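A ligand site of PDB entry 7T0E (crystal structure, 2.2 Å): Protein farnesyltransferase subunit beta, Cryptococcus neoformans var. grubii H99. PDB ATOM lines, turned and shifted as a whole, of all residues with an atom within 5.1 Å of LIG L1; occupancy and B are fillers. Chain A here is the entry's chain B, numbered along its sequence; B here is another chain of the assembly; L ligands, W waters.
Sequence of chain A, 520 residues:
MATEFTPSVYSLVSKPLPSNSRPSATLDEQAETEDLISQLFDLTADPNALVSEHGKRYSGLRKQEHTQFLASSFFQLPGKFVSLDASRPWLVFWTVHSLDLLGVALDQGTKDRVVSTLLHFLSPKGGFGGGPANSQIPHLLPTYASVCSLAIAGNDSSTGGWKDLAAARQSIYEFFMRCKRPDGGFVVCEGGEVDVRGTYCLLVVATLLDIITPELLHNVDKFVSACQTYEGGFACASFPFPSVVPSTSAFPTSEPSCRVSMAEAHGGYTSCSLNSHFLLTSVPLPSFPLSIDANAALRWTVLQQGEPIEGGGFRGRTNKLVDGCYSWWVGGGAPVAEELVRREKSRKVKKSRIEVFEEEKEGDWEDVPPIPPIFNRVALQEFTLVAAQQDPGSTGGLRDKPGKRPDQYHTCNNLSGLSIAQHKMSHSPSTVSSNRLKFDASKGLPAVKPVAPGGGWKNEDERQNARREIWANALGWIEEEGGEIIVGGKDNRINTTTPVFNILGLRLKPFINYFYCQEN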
ATOM      1  N   TRP A  90       2.708  15.849   4.021  1.00  0.00           N
ATOM      2  CA  TRP A  90       1.743  15.433   3.019  1.00  0.00           C
ATOM      3  C   TRP A  90       1.716  13.910   2.868  1.00  0.00           C
ATOM      4  O   TRP A  90       0.647  13.327   2.670  1.00  0.00           O
ATOM      5  CB  TRP A  90       2.036  16.102   1.687  1.00  0.00           C
ATOM      6  CG  TRP A  90       1.665  17.543   1.676  1.00  0.00           C
ATOM      7  CD1 TRP A  90       2.502  18.607   1.797  1.00  0.00           C
ATOM      8  CD2 TRP A  90       0.346  18.075   1.569  1.00  0.00           C
ATOM      9  NE1 TRP A  90       1.791  19.780   1.757  1.00  0.00           N
ATOM     10  CE2 TRP A  90       0.462  19.486   1.626  1.00  0.00           C
ATOM     11  CE3 TRP A  90      -0.929  17.515   1.433  1.00  0.00           C
ATOM     12  CZ2 TRP A  90      -0.641  20.323   1.541  1.00  0.00           C
ATOM     13  CZ3 TRP A  90      -2.024  18.352   1.354  1.00  0.00           C
ATOM     14  CH2 TRP A  90      -1.877  19.746   1.404  1.00  0.00           C
ATOM     15  N   LEU A 141       1.824  25.109   3.533  1.00  0.00           N
ATOM     16  CA  LEU A 141       1.226  23.875   3.024  1.00  0.00           C
ATOM     17  C   LEU A 141       1.473  22.699   3.961  1.00  0.00           C
ATOM     18  O   LEU A 141       0.528  21.965   4.274  1.00  0.00           O
ATOM     19  CB  LEU A 141       1.727  23.580   1.607  1.00  0.00           C
ATOM     20  CG  LEU A 141       0.894  24.135   0.449  1.00  0.00           C
ATOM     21  CD1 LEU A 141       0.783  25.660   0.516  1.00  0.00           C
ATOM     22  CD2 LEU A 141       1.470  23.707  -0.886  1.00  0.00           C
ATOM     23  N   ARG A 197      -3.307  28.364  -2.980  1.00  0.00           N
ATOM     24  CA  ARG A 197      -3.019  27.213  -2.124  1.00  0.00           C
ATOM     25  C   ARG A 197      -2.655  27.673  -0.719  1.00  0.00           C
ATOM     26  O   ARG A 197      -3.098  27.075   0.275  1.00  0.00           O
ATOM     27  CB  ARG A 197      -1.887  26.366  -2.690  1.00  0.00           C
ATOM     28  CG  ARG A 197      -2.100  25.753  -4.058  1.00  0.00           C
ATOM     29  CD  ARG A 197      -0.777  25.188  -4.524  1.00  0.00           C
ATOM     30  NE  ARG A 197       0.295  26.170  -4.343  1.00  0.00           N
ATOM     31  CZ  ARG A 197       1.586  25.893  -4.231  1.00  0.00           C
ATOM     32  NH1 ARG A 197       1.995  24.629  -4.266  1.00  0.00           N
ATOM     33  NH2 ARG A 197       2.462  26.868  -4.064  1.00  0.00           N
ATOM     34  N   TYR A 200      -5.821  29.016   1.037  1.00  0.00           N
ATOM     35  CA  TYR A 200      -6.677  27.915   1.460  1.00  0.00           C
ATOM     36  C   TYR A 200      -6.122  27.234   2.702  1.00  0.00           C
ATOM     37  O   TYR A 200      -6.821  27.078   3.711  1.00  0.00           O
ATOM     38  CB  TYR A 200      -6.842  26.910   0.330  1.00  0.00           C
ATOM     39  CG  TYR A 200      -7.410  25.586   0.793  1.00  0.00           C
ATOM     40  CD1 TYR A 200      -8.751  25.453   1.103  1.00  0.00           C
ATOM     41  CD2 TYR A 200      -6.591  24.465   0.954  1.00  0.00           C
ATOM     42  CE1 TYR A 200      -9.280  24.254   1.536  1.00  0.00           C
ATOM     43  CE2 TYR A 200      -7.107  23.260   1.387  1.00  0.00           C
ATOM     44  CZ  TYR A 200      -8.453  23.152   1.671  1.00  0.00           C
ATOM     45  OH  TYR A 200      -8.966  21.955   2.100  1.00  0.00           O
ATOM     46  N   CYS A 201      -4.859  26.808   2.641  1.00  0.00           N
ATOM     47  CA  CYS A 201      -4.241  26.130   3.777  1.00  0.00           C
ATOM     48  C   CYS A 201      -4.289  26.996   5.023  1.00  0.00           C
ATOM     49  O   CYS A 201      -4.582  26.494   6.118  1.00  0.00           O
ATOM     50  CB  CYS A 201      -2.800  25.747   3.435  1.00  0.00           C
ATOM     51  SG  CYS A 201      -2.638  24.430   2.204  1.00  0.00           S
ATOM     52  N   HIS A 266      -7.855  26.557 -13.232  1.00  0.00           N
ATOM     53  CA  HIS A 266      -7.358  25.206 -13.011  1.00  0.00           C
ATOM     54  C   HIS A 266      -8.115  24.573 -11.855  1.00  0.00           C
ATOM     55  O   HIS A 266      -8.493  25.250 -10.901  1.00  0.00           O
ATOM     56  CB  HIS A 266      -5.850  25.197 -12.736  1.00  0.00           C
ATOM     57  CG  HIS A 266      -5.236  23.835 -12.768  1.00  0.00           C
ATOM     58  ND1 HIS A 266      -5.288  22.963 -11.701  1.00  0.00           N
ATOM     59  CD2 HIS A 266      -4.551  23.193 -13.750  1.00  0.00           C
ATOM     60  CE1 HIS A 266      -4.657  21.843 -12.020  1.00  0.00           C
ATOM     61  NE2 HIS A 266      -4.203  21.954 -13.251  1.00  0.00           N
ATOM     62  N   GLY A 268      -7.226  22.572  -9.419  1.00  0.00           N
ATOM     63  CA  GLY A 268      -6.610  22.709  -8.103  1.00  0.00           C
ATOM     64  C   GLY A 268      -6.827  24.088  -7.499  1.00  0.00           C
ATOM     65  O   GLY A 268      -7.267  24.208  -6.346  1.00  0.00           O
ATOM     66  N   TYR A 269      -6.542  25.136  -8.265  1.00  0.00           N
ATOM     67  CA  TYR A 269      -6.700  26.492  -7.748  1.00  0.00           C
ATOM     68  C   TYR A 269      -8.157  26.898  -7.656  1.00  0.00           C
ATOM     69  O   TYR A 269      -8.515  27.750  -6.836  1.00  0.00           O
ATOM     70  CB  TYR A 269      -5.919  27.480  -8.616  1.00  0.00           C
ATOM     71  CG  TYR A 269      -4.426  27.210  -8.625  1.00  0.00           C
ATOM     72  CD1 TYR A 269      -3.694  27.297  -7.451  1.00  0.00           C
ATOM     73  CD2 TYR A 269      -3.762  26.860  -9.784  1.00  0.00           C
ATOM     74  CE1 TYR A 269      -2.341  27.042  -7.432  1.00  0.00           C
ATOM     75  CE2 TYR A 269      -2.404  26.615  -9.785  1.00  0.00           C
ATOM     76  CZ  TYR A 269      -1.694  26.705  -8.601  1.00  0.00           C
ATOM     77  OH  TYR A 269      -0.348  26.469  -8.572  1.00  0.00           O
ATOM     78  N   CYS A 272      -9.156  25.503  -4.207  1.00  0.00           N
ATOM     79  CA  CYS A 272      -8.657  26.353  -3.123  1.00  0.00           C
ATOM     80  C   CYS A 272      -9.409  27.680  -3.064  1.00  0.00           C
ATOM     81  O   CYS A 272      -9.674  28.206  -1.981  1.00  0.00           O
ATOM     82  CB  CYS A 272      -7.164  26.605  -3.287  1.00  0.00           C
ATOM     83  SG  CYS A 272      -6.141  25.117  -3.155  1.00  0.00           S
ATOM     84  N   GLY A 316      -8.339  18.864 -15.229  1.00  0.00           N
ATOM     85  CA  GLY A 316      -7.979  20.024 -14.431  1.00  0.00           C
ATOM     86  C   GLY A 316      -8.159  21.351 -15.134  1.00  0.00           C
ATOM     87  O   GLY A 316      -8.349  22.380 -14.485  1.00  0.00           O
ATOM     88  N   ARG A 317      -8.088  21.344 -16.467  1.00  0.00           N
ATOM     89  CA  ARG A 317      -8.310  22.575 -17.229  1.00  0.00           C
ATOM     90  C   ARG A 317      -8.754  22.212 -18.629  1.00  0.00           C
ATOM     91  O   ARG A 317      -8.604  21.070 -19.088  1.00  0.00           O
ATOM     92  CB  ARG A 317      -7.053  23.454 -17.258  1.00  0.00           C
ATOM     93  CG  ARG A 317      -5.743  22.706 -17.299  1.00  0.00           C
ATOM     94  CD  ARG A 317      -4.544  23.649 -17.368  1.00  0.00           C
ATOM     95  NE  ARG A 317      -3.296  22.948 -17.111  1.00  0.00           N
ATOM     96  CZ  ARG A 317      -2.098  23.376 -17.482  1.00  0.00           C
ATOM     97  NH1 ARG A 317      -1.964  24.519 -18.142  1.00  0.00           N
ATOM     98  NH2 ARG A 317      -1.015  22.650 -17.199  1.00  0.00           N
ATOM     99  N   LYS A 320      -7.168  19.785 -21.605  1.00  0.00           N
ATOM    100  CA  LYS A 320      -6.171  18.907 -21.012  1.00  0.00           C
ATOM    101  C   LYS A 320      -6.809  17.547 -20.747  1.00  0.00           C
ATOM    102  O   LYS A 320      -7.956  17.289 -21.148  1.00  0.00           O
ATOM    103  CB  LYS A 320      -5.585  19.546 -19.751  1.00  0.00           C
ATOM    104  CG  LYS A 320      -4.612  20.682 -20.032  1.00  0.00           C
ATOM    105  CD  LYS A 320      -3.291  20.148 -20.558  1.00  0.00           C
ATOM    106  CE  LYS A 320      -2.142  20.511 -19.624  1.00  0.00           C
ATOM    107  NZ  LYS A 320      -1.134  19.416 -19.534  1.00  0.00           N
ATOM    108  N   LEU A 321      -6.083  16.667 -20.078  1.00  0.00           N
ATOM    109  CA  LEU A 321      -6.485  15.268 -19.927  1.00  0.00           C
ATOM    110  C   LEU A 321      -7.172  15.025 -18.586  1.00  0.00           C
ATOM    111  O   LEU A 321      -6.877  15.691 -17.585  1.00  0.00           O
ATOM    112  CB  LEU A 321      -5.273  14.348 -20.054  1.00  0.00           C
ATOM    113  CG  LEU A 321      -4.416  14.484 -21.320  1.00  0.00           C
ATOM    114  CD1 LEU A 321      -3.229  13.539 -21.260  1.00  0.00           C
ATOM    115  CD2 LEU A 321      -5.241  14.253 -22.570  1.00  0.00           C
ATOM    116  N   ASP A 323      -7.925  13.199 -15.092  1.00  0.00           N
ATOM    117  CA  ASP A 323      -6.975  12.742 -14.093  1.00  0.00           C
ATOM    118  C   ASP A 323      -7.748  12.427 -12.822  1.00  0.00           C
ATOM    119  O   ASP A 323      -8.554  13.245 -12.369  1.00  0.00           O
ATOM    120  CB  ASP A 323      -5.897  13.807 -13.840  1.00  0.00           C
ATOM    121  CG  ASP A 323      -4.821  13.375 -12.852  1.00  0.00           C
ATOM    122  OD1 ASP A 323      -5.111  12.595 -11.920  1.00  0.00           O
ATOM    123  OD2 ASP A 323      -3.672  13.828 -13.005  1.00  0.00           O
ATOM    124  N   TYR A 326      -8.317  14.892  -9.840  1.00  0.00           N
ATOM    125  CA  TYR A 326      -9.284  15.972  -9.947  1.00  0.00           C
ATOM    126  C   TYR A 326     -10.697  15.548  -9.584  1.00  0.00           C
ATOM    127  O   TYR A 326     -11.615  16.384  -9.610  1.00  0.00           O
ATOM    128  CB  TYR A 326      -9.272  16.562 -11.362  1.00  0.00           C
ATOM    129  CG  TYR A 326      -7.939  17.158 -11.738  1.00  0.00           C
ATOM    130  CD1 TYR A 326      -7.365  18.153 -10.965  1.00  0.00           C
ATOM    131  CD2 TYR A 326      -7.252  16.719 -12.863  1.00  0.00           C
ATOM    132  CE1 TYR A 326      -6.141  18.695 -11.303  1.00  0.00           C
ATOM    133  CE2 TYR A 326      -6.035  17.260 -13.208  1.00  0.00           C
ATOM    134  CZ  TYR A 326      -5.481  18.244 -12.426  1.00  0.00           C
ATOM    135  OH  TYR A 326      -4.257  18.786 -12.764  1.00  0.00           O
ATOM    136  N   TRP A 329     -10.399  17.576  -6.496  1.00  0.00           N
ATOM    137  CA  TRP A 329     -10.191  19.006  -6.724  1.00  0.00           C
ATOM    138  C   TRP A 329     -11.399  19.647  -7.392  1.00  0.00           C
ATOM    139  O   TRP A 329     -11.915  20.672  -6.929  1.00  0.00           O
ATOM    140  CB  TRP A 329      -8.927  19.238  -7.539  1.00  0.00           C
ATOM    141  CG  TRP A 329      -7.669  18.768  -6.868  1.00  0.00           C
ATOM    142  CD1 TRP A 329      -6.764  17.875  -7.362  1.00  0.00           C
ATOM    143  CD2 TRP A 329      -7.174  19.161  -5.577  1.00  0.00           C
ATOM    144  NE1 TRP A 329      -5.745  17.686  -6.461  1.00  0.00           N
ATOM    145  CE2 TRP A 329      -5.973  18.460  -5.358  1.00  0.00           C
ATOM    146  CE3 TRP A 329      -7.639  20.047  -4.594  1.00  0.00           C
ATOM    147  CZ2 TRP A 329      -5.219  18.616  -4.195  1.00  0.00           C
ATOM    148  CZ3 TRP A 329      -6.891  20.189  -3.439  1.00  0.00           C
ATOM    149  CH2 TRP A 329      -5.695  19.477  -3.246  1.00  0.00           C
ATOM    150  N   TYR A 409      -0.421  10.460  -3.317  1.00  0.00           N
ATOM    151  CA  TYR A 409      -1.211  11.651  -3.623  1.00  0.00           C
ATOM    152  C   TYR A 409      -2.467  11.288  -4.412  1.00  0.00           C
ATOM    153  O   TYR A 409      -3.570  11.742  -4.073  1.00  0.00           O
ATOM    154  CB  TYR A 409      -0.358  12.660  -4.389  1.00  0.00           C
ATOM    155  CG  TYR A 409      -1.159  13.708  -5.124  1.00  0.00           C
ATOM    156  CD1 TYR A 409      -1.629  14.838  -4.465  1.00  0.00           C
ATOM    157  CD2 TYR A 409      -1.432  13.583  -6.480  1.00  0.00           C
ATOM    158  CE1 TYR A 409      -2.357  15.804  -5.132  1.00  0.00           C
ATOM    159  CE2 TYR A 409      -2.162  14.544  -7.161  1.00  0.00           C
ATOM    160  CZ  TYR A 409      -2.619  15.651  -6.486  1.00  0.00           C
ATOM    161  OH  TYR A 409      -3.350  16.609  -7.149  1.00  0.00           O
ATOM    162  N   TYR B 123       8.077  24.303  -8.216  1.00  0.00           N
ATOM    163  CA  TYR B 123       7.618  25.622  -7.789  1.00  0.00           C
ATOM    164  C   TYR B 123       8.789  26.491  -7.351  1.00  0.00           C
ATOM    165  O   TYR B 123       8.793  27.700  -7.569  1.00  0.00           O
ATOM    166  CB  TYR B 123       6.636  25.486  -6.624  1.00  0.00           C
ATOM    167  CG  TYR B 123       5.209  25.165  -6.983  1.00  0.00           C
ATOM    168  CD1 TYR B 123       4.310  26.176  -7.331  1.00  0.00           C
ATOM    169  CD2 TYR B 123       4.739  23.861  -6.939  1.00  0.00           C
ATOM    170  CE1 TYR B 123       2.995  25.883  -7.638  1.00  0.00           C
ATOM    171  CE2 TYR B 123       3.429  23.562  -7.252  1.00  0.00           C
ATOM    172  CZ  TYR B 123       2.562  24.576  -7.592  1.00  0.00           C
ATOM    173  OH  TYR B 123       1.253  24.276  -7.904  1.00  0.00           O
ATOM    174  N   TYR B 159       2.044  25.216 -16.687  1.00  0.00           N
ATOM    175  CA  TYR B 159       1.266  26.203 -15.953  1.00  0.00           C
ATOM    176  C   TYR B 159       2.161  27.230 -15.271  1.00  0.00           C
ATOM    177  O   TYR B 159       1.861  28.426 -15.276  1.00  0.00           O
ATOM    178  CB  TYR B 159       0.354  25.515 -14.939  1.00  0.00           C
ATOM    179  CG  TYR B 159      -0.709  26.434 -14.363  1.00  0.00           C
ATOM    180  CD1 TYR B 159      -0.422  27.274 -13.287  1.00  0.00           C
ATOM    181  CD2 TYR B 159      -1.987  26.462 -14.901  1.00  0.00           C
ATOM    182  CE1 TYR B 159      -1.385  28.121 -12.769  1.00  0.00           C
ATOM    183  CE2 TYR B 159      -2.956  27.294 -14.392  1.00  0.00           C
ATOM    184  CZ  TYR B 159      -2.651  28.124 -13.323  1.00  0.00           C
ATOM    185  OH  TYR B 159      -3.620  28.957 -12.814  1.00  0.00           O
ATOM    186  N   HIS B 160       3.263  26.772 -14.662  1.00  0.00           N
ATOM    187  CA  HIS B 160       4.175  27.697 -14.002  1.00  0.00           C
ATOM    188  C   HIS B 160       4.754  28.699 -14.986  1.00  0.00           C
ATOM    189  O   HIS B 160       4.910  29.894 -14.663  1.00  0.00           O
ATOM    190  CB  HIS B 160       5.316  26.937 -13.316  1.00  0.00           C
ATOM    191  CG  HIS B 160       4.844  25.861 -12.384  1.00  0.00           C
ATOM    192  ND1 HIS B 160       4.986  24.519 -12.677  1.00  0.00           N
ATOM    193  CD2 HIS B 160       4.246  25.918 -11.182  1.00  0.00           C
ATOM    194  CE1 HIS B 160       4.490  23.799 -11.683  1.00  0.00           C
ATOM    195  NE2 HIS B 160       4.037  24.623 -10.762  1.00  0.00           N
HETATM  196  C1  LIG L   1      -0.823  21.524 -13.244  1.00  0.00           C
HETATM  197  O1  LIG L   1       0.198  20.593 -13.455  1.00  0.00           O
HETATM  198  C2  LIG L   1      -0.232  22.793 -12.648  1.00  0.00           C
HETATM  199  C3  LIG L   1      -0.498  23.137 -11.407  1.00  0.00           C
HETATM  200  C4  LIG L   1       0.128  24.418 -10.853  1.00  0.00           C
HETATM  201  C5  LIG L   1      -1.405  22.252 -10.559  1.00  0.00           C
HETATM  202  C6  LIG L   1      -1.896  22.874  -9.246  1.00  0.00           C
HETATM  203  C7  LIG L   1      -2.764  21.762  -8.667  1.00  0.00           C
HETATM  204  C8  LIG L   1      -3.299  21.660  -7.463  1.00  0.00           C
HETATM  205  C9  LIG L   1      -4.109  20.404  -7.210  1.00  0.00           C
HETATM  206  C10 LIG L   1      -3.165  22.684  -6.344  1.00  0.00           C
HETATM  207  C11 LIG L   1      -2.893  21.916  -5.040  1.00  0.00           C
HETATM  208  C12 LIG L   1      -3.779  22.376  -3.877  1.00  0.00           C
HETATM  209  C13 LIG L   1      -3.318  22.298  -2.642  1.00  0.00           C
HETATM  210  C14 LIG L   1      -4.172  22.744  -1.456  1.00  0.00           C
HETATM  211  C15 LIG L   1      -1.917  21.756  -2.367  1.00  0.00           C
HETATM  212  P1  LIG L   1       0.031  19.494 -14.677  1.00  0.00           P
HETATM  213  O2  LIG L   1       0.174  20.208 -15.999  1.00  0.00           O
HETATM  214  O3  LIG L   1       1.094  18.422 -14.546  1.00  0.00           O
HETATM  215  O4  LIG L   1      -1.464  18.813 -14.578  1.00  0.00           O
HETATM  216  P2  LIG L   1      -2.674  19.099 -15.656  1.00  0.00           P
HETATM  217  O5  LIG L   1      -2.171  18.843 -17.044  1.00  0.00           O
HETATM  218  O6  LIG L   1      -3.147  20.535 -15.527  1.00  0.00           O
HETATM  219  O7  LIG L   1      -3.835  18.169 -15.365  1.00  0.00           O
HETATM  220  C1  LG2 L   2       3.943  18.082  -2.629  1.00  0.00           C
HETATM  221  C2  LG2 L   2       3.369  17.743  -7.105  1.00  0.00           C
HETATM  222  C3  LG2 L   2       3.178  17.147  -8.563  1.00  0.00           C
HETATM  223  C4  LG2 L   2       0.367  15.929 -10.362  1.00  0.00           C
HETATM  224  C5  LG2 L   2      -0.365  14.734 -10.393  1.00  0.00           C
HETATM  225  C6  LG2 L   2       0.029  19.058  -9.426  1.00  0.00           C
HETATM  226  C7  LG2 L   2       1.199  20.691  -8.066  1.00  0.00           C
HETATM  227  C8  LG2 L   2       3.506  11.669  -5.071  1.00  0.00           C
HETATM  228  C9  LG2 L   2       3.776  12.407  -6.404  1.00  0.00           C
HETATM  229  C10 LG2 L   2       2.545  13.203  -6.885  1.00  0.00           C
HETATM  230  C11 LG2 L   2       2.922  14.451  -7.794  1.00  0.00           C
HETATM  231  C12 LG2 L   2       1.732  15.549  -7.819  1.00  0.00           C
HETATM  232  C13 LG2 L   2       1.587  16.100  -6.425  1.00  0.00           C
HETATM  233  C14 LG2 L   2       2.632  17.632  -4.614  1.00  0.00           C
HETATM  234  C15 LG2 L   2       3.853  17.629  -3.957  1.00  0.00           C
HETATM  235  C16 LG2 L   2       2.808  18.527  -1.983  1.00  0.00           C
HETATM  236  C17 LG2 L   2       1.576  18.522  -2.641  1.00  0.00           C
HETATM  237  C18 LG2 L   2       1.492  18.083  -3.961  1.00  0.00           C
HETATM  238  C19 LG2 L   2       1.893  16.069  -9.968  1.00  0.00           C
HETATM  239  C20 LG2 L   2      -1.691  16.382 -10.957  1.00  0.00           C
HETATM  240  C21 LG2 L   2      -0.171  18.387 -10.827  1.00  0.00           C
HETATM  241  C22 LG2 L   2       0.991  20.072  -9.300  1.00  0.00           C
HETATM  242  C23 LG2 L   2       0.442  20.326  -6.972  1.00  0.00           C
HETATM  243  C24 LG2 L   2      -0.520  19.313  -7.098  1.00  0.00           C
HETATM  244  C25 LG2 L   2      -0.726  18.680  -8.334  1.00  0.00           C
HETATM  245  N1  LG2 L   2       2.532  17.157  -6.040  1.00  0.00           N
HETATM  246  N2  LG2 L   2       1.978  16.547  -8.759  1.00  0.00           N
HETATM  247  N3  LG2 L   2      -1.623  15.056 -10.765  1.00  0.00           N
HETATM  248  N4  LG2 L   2      -0.497  16.915 -10.707  1.00  0.00           N
HETATM  249  O1  LG2 L   2       4.159  18.605  -6.879  1.00  0.00           O
HETATM  250 BR1  LG2 L   2       0.743  21.208  -5.267  1.00  0.00          BR
HETATM  251 CL1  LG2 L   2       0.106  19.098  -1.807  1.00  0.00          CL
HETATM  252  O   HOH W   1       3.179  18.984 -12.353  1.00  0.00           O
HETATM  253  O   HOH W   2      -0.085  16.163 -14.116  1.00  0.00           O
HETATM  254  O   HOH W   3      -6.084  18.194 -16.739  1.00  0.00           O
HETATM  255  O   HOH W   4      -3.550  17.012 -18.496  1.00  0.00           O
HETATM  256  O   HOH W   5      -2.884  15.760 -14.932  1.00  0.00           O
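The side-chain hydroxyl of Tyr 326 sits at hydrogen-bond distance from an oxygen (O7) of LIG L1 (2.7 Å). An oxygen (O5) of LIG L1 lies within salt-bridge range of the side-chain amino group (NZ) of Lys 320 (2.8 Å). A ring nitrogen (NE2) of His 266 is in hydrogen-bond range of an oxygen (O6) of LIG L1 (2.9 Å). O6 of LIG L1 lies within salt-bridge range of NE of Arg 317.
Water W3 lies within hydrogen-bond range of an oxygen (O7) of LIG L1 (2.6 Å), the backbone carbonyl oxygen (O) of Leu 321 (2.8 Å) and the backbone NH (N) of Gly 316 (2.8 Å). Water W4 bridges O5 of LIG L1 (2.7 Å) and N of Leu 321 (3.0 Å).
Merely in contact with LIG L1: Tyr 269 (3.1 Å), Tyr 123 of chain B (3.2 Å), Trp 329 (3.3 Å), Gly 268 (3.5 Å), Cys 272 (3.5 Å), Tyr 159 of chain B (3.6 Å), Arg 197 (3.8 Å), Tyr 200 (3.8 Å), Tyr 409 (3.9 Å) and His 160 of chain B (3.9 Å). Hydrophobic or aromatic side chains that line LIG L1: Tyr 200, His 266, Tyr 269, Tyr 326, Trp 329 and Tyr 159 of chain B. Along chain A the residues within 4 Å of LIG L1 span positions 197 to 409. The nearest printed residue that does not touch LIG L1 is Leu 141 (4.2 Å).
A ring nitrogen (NE2) of His 266 sits close to the side-chain hydroxyl (OH) of Tyr 326 (3.2 Å). ND1 of His 266 sits at hydrogen-bond distance from N of Gly 268, at 3.0 Å. The side-chain hydroxyl (OH) of Tyr 123 of chain B lies within hydrogen-bond range of the side-chain hydroxyl (OH) of Tyr 269. The side-chain hydroxyl (OH) of Tyr 409 is in hydrogen-bond range of the indole nitrogen (NE1) of Trp 329, 2.7 Å away. The backbone carbonyl oxygen (O) of Gly 268 is in hydrogen-bond range of the side-chain sulfur (SG) of Cys 272 (3.5 Å). The side-chain sulfur of Cys 201 sits at hydrogen-bond distance from the backbone carbonyl oxygen of Arg 197 (3.3 Å).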
